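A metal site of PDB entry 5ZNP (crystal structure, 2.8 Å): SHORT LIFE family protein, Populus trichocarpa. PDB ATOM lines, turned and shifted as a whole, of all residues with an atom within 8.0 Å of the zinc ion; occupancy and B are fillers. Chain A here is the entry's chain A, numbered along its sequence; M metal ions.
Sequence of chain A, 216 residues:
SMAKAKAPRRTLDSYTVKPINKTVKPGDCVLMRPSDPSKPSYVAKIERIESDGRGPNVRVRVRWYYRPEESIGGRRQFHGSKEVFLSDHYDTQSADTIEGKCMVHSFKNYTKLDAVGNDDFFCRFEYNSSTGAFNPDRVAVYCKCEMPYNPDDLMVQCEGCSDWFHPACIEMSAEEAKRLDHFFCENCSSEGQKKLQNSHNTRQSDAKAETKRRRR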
ATOM      1  N   GLN A  77      18.561 -23.103  12.272  1.00  0.00           N
ATOM      2  CA  GLN A  77      18.495 -22.015  11.298  1.00  0.00           C
ATOM      3  C   GLN A  77      18.382 -20.629  11.937  1.00  0.00           C
ATOM      4  O   GLN A  77      19.015 -19.674  11.476  1.00  0.00           O
ATOM      5  CB  GLN A  77      17.304 -22.240  10.364  1.00  0.00           C
ATOM      6  CG  GLN A  77      16.018 -22.583  11.106  1.00  0.00           C
ATOM      7  CD  GLN A  77      14.824 -22.716  10.192  1.00  0.00           C
ATOM      8  OE1 GLN A  77      14.947 -22.604   8.972  1.00  0.00           O
ATOM      9  NE2 GLN A  77      13.660 -22.949  10.781  1.00  0.00           N
ATOM     10  N   TYR A 142       8.341 -14.987  13.463  1.00  0.00           N
ATOM     11  CA  TYR A 142       7.982 -14.105  12.359  1.00  0.00           C
ATOM     12  C   TYR A 142       7.900 -14.830  11.016  1.00  0.00           C
ATOM     13  O   TYR A 142       8.287 -15.984  10.908  1.00  0.00           O
ATOM     14  CB  TYR A 142       8.986 -12.951  12.259  1.00  0.00           C
ATOM     15  CG  TYR A 142       9.249 -12.255  13.575  1.00  0.00           C
ATOM     16  CD1 TYR A 142      10.356 -12.609  14.352  1.00  0.00           C
ATOM     17  CD2 TYR A 142       8.399 -11.268  14.045  1.00  0.00           C
ATOM     18  CE1 TYR A 142      10.596 -11.982  15.554  1.00  0.00           C
ATOM     19  CE2 TYR A 142       8.639 -10.634  15.259  1.00  0.00           C
ATOM     20  CZ  TYR A 142       9.739 -11.007  16.006  1.00  0.00           C
ATOM     21  OH  TYR A 142       9.979 -10.379  17.208  1.00  0.00           O
ATOM     22  N   CYS A 143       7.380 -14.130  10.010  1.00  0.00           N
ATOM     23  CA  CYS A 143       7.251 -14.626   8.635  1.00  0.00           C
ATOM     24  C   CYS A 143       6.361 -15.865   8.529  1.00  0.00           C
ATOM     25  O   CYS A 143       5.766 -16.293   9.521  1.00  0.00           O
ATOM     26  CB  CYS A 143       8.641 -14.930   8.053  1.00  0.00           C
ATOM     27  SG  CYS A 143       8.633 -15.342   6.296  1.00  0.00           S
ATOM     28  N   LYS A 144       6.264 -16.430   7.331  1.00  0.00           N
ATOM     29  CA  LYS A 144       5.428 -17.608   7.109  1.00  0.00           C
ATOM     30  C   LYS A 144       6.099 -18.856   7.652  1.00  0.00           C
ATOM     31  O   LYS A 144       5.431 -19.843   7.985  1.00  0.00           O
ATOM     32  CB  LYS A 144       5.125 -17.808   5.634  1.00  0.00           C
ATOM     33  CG  LYS A 144       4.909 -16.541   4.838  1.00  0.00           C
ATOM     34  CD  LYS A 144       4.604 -16.889   3.390  1.00  0.00           C
ATOM     35  CE  LYS A 144       5.546 -17.965   2.855  1.00  0.00           C
ATOM     36  NZ  LYS A 144       6.983 -17.620   3.019  1.00  0.00           N
ATOM     37  N   CYS A 145       7.420 -18.827   7.745  1.00  0.00           N
ATOM     38  CA  CYS A 145       8.168 -19.918   8.335  1.00  0.00           C
ATOM     39  C   CYS A 145       7.852 -20.007   9.821  1.00  0.00           C
ATOM     40  O   CYS A 145       8.046 -21.048  10.449  1.00  0.00           O
ATOM     41  CB  CYS A 145       9.678 -19.730   8.116  1.00  0.00           C
ATOM     42  SG  CYS A 145      10.326 -18.142   8.669  1.00  0.00           S
ATOM     43  N   GLU A 146       7.357 -18.892  10.367  1.00  0.00           N
ATOM     44  CA  GLU A 146       7.000 -18.775  11.778  1.00  0.00           C
ATOM     45  C   GLU A 146       8.129 -19.268  12.673  1.00  0.00           C
ATOM     46  O   GLU A 146       7.939 -20.118  13.532  1.00  0.00           O
ATOM     47  CB  GLU A 146       5.697 -19.526  12.069  1.00  0.00           C
ATOM     48  CG  GLU A 146       4.479 -18.899  11.399  1.00  0.00           C
ATOM     49  CD  GLU A 146       3.171 -19.326  12.019  1.00  0.00           C
ATOM     50  OE1 GLU A 146       2.980 -20.542  12.248  1.00  0.00           O
ATOM     51  OE2 GLU A 146       2.323 -18.445  12.280  1.00  0.00           O
ATOM     52  N   MET A 147       9.310 -18.713  12.422  1.00  0.00           N
ATOM     53  CA  MET A 147      10.520 -19.056  13.167  1.00  0.00           C
ATOM     54  C   MET A 147      11.019 -17.839  13.933  1.00  0.00           C
ATOM     55  O   MET A 147      10.742 -16.707  13.555  1.00  0.00           O
ATOM     56  CB  MET A 147      11.605 -19.571  12.223  1.00  0.00           C
ATOM     57  CG  MET A 147      11.258 -20.880  11.515  1.00  0.00           C
ATOM     58  SD  MET A 147      11.651 -22.332  12.502  1.00  0.00           S
ATOM     59  CE  MET A 147      10.058 -22.705  13.226  1.00  0.00           C
ATOM     60  N   PRO A 148      11.754 -18.074  15.038  1.00  0.00           N
ATOM     61  CA  PRO A 148      12.396 -16.986  15.777  1.00  0.00           C
ATOM     62  C   PRO A 148      13.388 -16.203  14.920  1.00  0.00           C
ATOM     63  O   PRO A 148      13.848 -16.700  13.894  1.00  0.00           O
ATOM     64  CB  PRO A 148      13.116 -17.702  16.919  1.00  0.00           C
ATOM     65  CG  PRO A 148      12.341 -18.966  17.103  1.00  0.00           C
ATOM     66  CD  PRO A 148      11.906 -19.362  15.733  1.00  0.00           C
ATOM     67  N   LEU A 154      18.254 -10.908   6.991  1.00  0.00           N
ATOM     68  CA  LEU A 154      17.553  -9.680   6.648  1.00  0.00           C
ATOM     69  C   LEU A 154      16.048  -9.921   6.507  1.00  0.00           C
ATOM     70  O   LEU A 154      15.618 -10.815   5.776  1.00  0.00           O
ATOM     71  CB  LEU A 154      18.103  -9.100   5.343  1.00  0.00           C
ATOM     72  CG  LEU A 154      17.597  -7.728   4.907  1.00  0.00           C
ATOM     73  CD1 LEU A 154      18.504  -6.626   5.423  1.00  0.00           C
ATOM     74  CD2 LEU A 154      17.457  -7.665   3.394  1.00  0.00           C
ATOM     75  N   MET A 155      15.264  -9.122   7.220  1.00  0.00           N
ATOM     76  CA  MET A 155      13.809  -9.177   7.104  1.00  0.00           C
ATOM     77  C   MET A 155      13.258  -7.811   6.712  1.00  0.00           C
ATOM     78  O   MET A 155      13.979  -6.813   6.753  1.00  0.00           O
ATOM     79  CB  MET A 155      13.174  -9.644   8.410  1.00  0.00           C
ATOM     80  CG  MET A 155      13.682 -10.990   8.913  1.00  0.00           C
ATOM     81  SD  MET A 155      12.884 -11.484  10.449  1.00  0.00           S
ATOM     82  CE  MET A 155      11.967 -12.918   9.902  1.00  0.00           C
ATOM     83  N   TRP A 164       7.416  -9.287   9.606  1.00  0.00           N
ATOM     84  CA  TRP A 164       8.678  -9.193   8.947  1.00  0.00           C
ATOM     85  C   TRP A 164       8.884 -10.457   8.165  1.00  0.00           C
ATOM     86  O   TRP A 164       8.470 -11.519   8.594  1.00  0.00           O
ATOM     87  CB  TRP A 164       9.779  -9.042   9.983  1.00  0.00           C
ATOM     88  CG  TRP A 164       9.722  -7.797  10.807  1.00  0.00           C
ATOM     89  CD1 TRP A 164       9.001  -7.602  11.934  1.00  0.00           C
ATOM     90  CD2 TRP A 164      10.414  -6.587  10.573  1.00  0.00           C
ATOM     91  NE1 TRP A 164       9.200  -6.357  12.412  1.00  0.00           N
ATOM     92  CE2 TRP A 164      10.075  -5.710  11.577  1.00  0.00           C
ATOM     93  CE3 TRP A 164      11.307  -6.179   9.597  1.00  0.00           C
ATOM     94  CZ2 TRP A 164      10.579  -4.443  11.648  1.00  0.00           C
ATOM     95  CZ3 TRP A 164      11.798  -4.930   9.662  1.00  0.00           C
ATOM     96  CH2 TRP A 164      11.439  -4.067  10.665  1.00  0.00           C
ATOM     97  N   PHE A 165       9.529 -10.343   7.033  1.00  0.00           N
ATOM     98  CA  PHE A 165       9.680 -11.494   6.180  1.00  0.00           C
ATOM     99  C   PHE A 165      11.082 -11.737   5.662  1.00  0.00           C
ATOM    100  O   PHE A 165      11.753 -10.818   5.269  1.00  0.00           O
ATOM    101  CB  PHE A 165       8.666 -11.393   5.049  1.00  0.00           C
ATOM    102  CG  PHE A 165       7.255 -11.383   5.528  1.00  0.00           C
ATOM    103  CD1 PHE A 165       6.742 -10.295   6.155  1.00  0.00           C
ATOM    104  CD2 PHE A 165       6.458 -12.474   5.387  1.00  0.00           C
ATOM    105  CE1 PHE A 165       5.463 -10.272   6.617  1.00  0.00           C
ATOM    106  CE2 PHE A 165       5.173 -12.464   5.848  1.00  0.00           C
ATOM    107  CZ  PHE A 165       4.673 -11.366   6.469  1.00  0.00           C
ATOM    108  N   HIS A 166      11.526 -12.990   5.650  1.00  0.00           N
ATOM    109  CA  HIS A 166      12.681 -13.349   4.836  1.00  0.00           C
ATOM    110  C   HIS A 166      12.264 -13.271   3.375  1.00  0.00           C
ATOM    111  O   HIS A 166      11.244 -13.838   2.997  1.00  0.00           O
ATOM    112  CB  HIS A 166      13.195 -14.743   5.170  1.00  0.00           C
ATOM    113  CG  HIS A 166      13.601 -14.931   6.604  1.00  0.00           C
ATOM    114  ND1 HIS A 166      12.916 -15.769   7.455  1.00  0.00           N
ATOM    115  CD2 HIS A 166      14.619 -14.396   7.317  1.00  0.00           C
ATOM    116  CE1 HIS A 166      13.496 -15.741   8.641  1.00  0.00           C
ATOM    117  NE2 HIS A 166      14.531 -14.918   8.582  1.00  0.00           N
ATOM    118  N   PRO A 167      13.054 -12.564   2.548  1.00  0.00           N
ATOM    119  CA  PRO A 167      12.766 -12.473   1.111  1.00  0.00           C
ATOM    120  C   PRO A 167      12.690 -13.846   0.451  1.00  0.00           C
ATOM    121  O   PRO A 167      11.755 -14.105  -0.314  1.00  0.00           O
ATOM    122  CB  PRO A 167      13.950 -11.682   0.579  1.00  0.00           C
ATOM    123  CG  PRO A 167      14.396 -10.848   1.734  1.00  0.00           C
ATOM    124  CD  PRO A 167      14.189 -11.716   2.936  1.00  0.00           C
ATOM    125  N   ALA A 168      13.655 -14.706   0.745  1.00  0.00           N
ATOM    126  CA  ALA A 168      13.711 -16.049   0.180  1.00  0.00           C
ATOM    127  C   ALA A 168      12.470 -16.859   0.512  1.00  0.00           C
ATOM    128  O   ALA A 168      12.029 -17.707  -0.277  1.00  0.00           O
ATOM    129  CB  ALA A 168      14.960 -16.771   0.652  1.00  0.00           C
ATOM    130  N   CYS A 169      11.904 -16.609   1.688  1.00  0.00           N
ATOM    131  CA  CYS A 169      10.684 -17.303   2.116  1.00  0.00           C
ATOM    132  C   CYS A 169       9.494 -16.930   1.233  1.00  0.00           C
ATOM    133  O   CYS A 169       8.523 -17.688   1.140  1.00  0.00           O
ATOM    134  CB  CYS A 169      10.371 -16.984   3.582  1.00  0.00           C
ATOM    135  SG  CYS A 169      11.452 -17.803   4.778  1.00  0.00           S
ATOM    136  N   ILE A 170       9.562 -15.770   0.591  1.00  0.00           N
ATOM    137  CA  ILE A 170       8.487 -15.340  -0.287  1.00  0.00           C
ATOM    138  C   ILE A 170       8.965 -14.789  -1.623  1.00  0.00           C
ATOM    139  O   ILE A 170       8.668 -13.649  -1.980  1.00  0.00           O
ATOM    140  CB  ILE A 170       7.605 -14.257   0.365  1.00  0.00           C
ATOM    141  CG1 ILE A 170       8.454 -13.285   1.183  1.00  0.00           C
ATOM    142  CG2 ILE A 170       6.552 -14.891   1.236  1.00  0.00           C
ATOM    143  CD1 ILE A 170       7.625 -12.268   1.928  1.00  0.00           C
HETATM  144 ZN    ZN M   1      10.705 -16.532   6.751  1.00  0.00          ZN
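O of Tyr 142 lies close to SG of Cys 145 (3.7 Å). NZ of Lys 144 sits at hydrogen-bond distance from O of Cys 169 (2.4 Å). The backbone carbonyl oxygen of Trp 164 lies within hydrogen-bond range of the backbone NH of Cys 143 (3.2 Å).
Within 4 Å of the zinc ion: Cys 143, Cys 145, His 166 and Cys 169.
SG of Cys 143 is bound to the zinc ion (2.4 Å). The zinc ion is bound by a ring nitrogen (ND1) of His 166 (2.4 Å). The zinc ion is bound by SG of Cys 169 (2.5 Å). SG of Cys 145 binds the zinc ion, at 2.5 Å.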
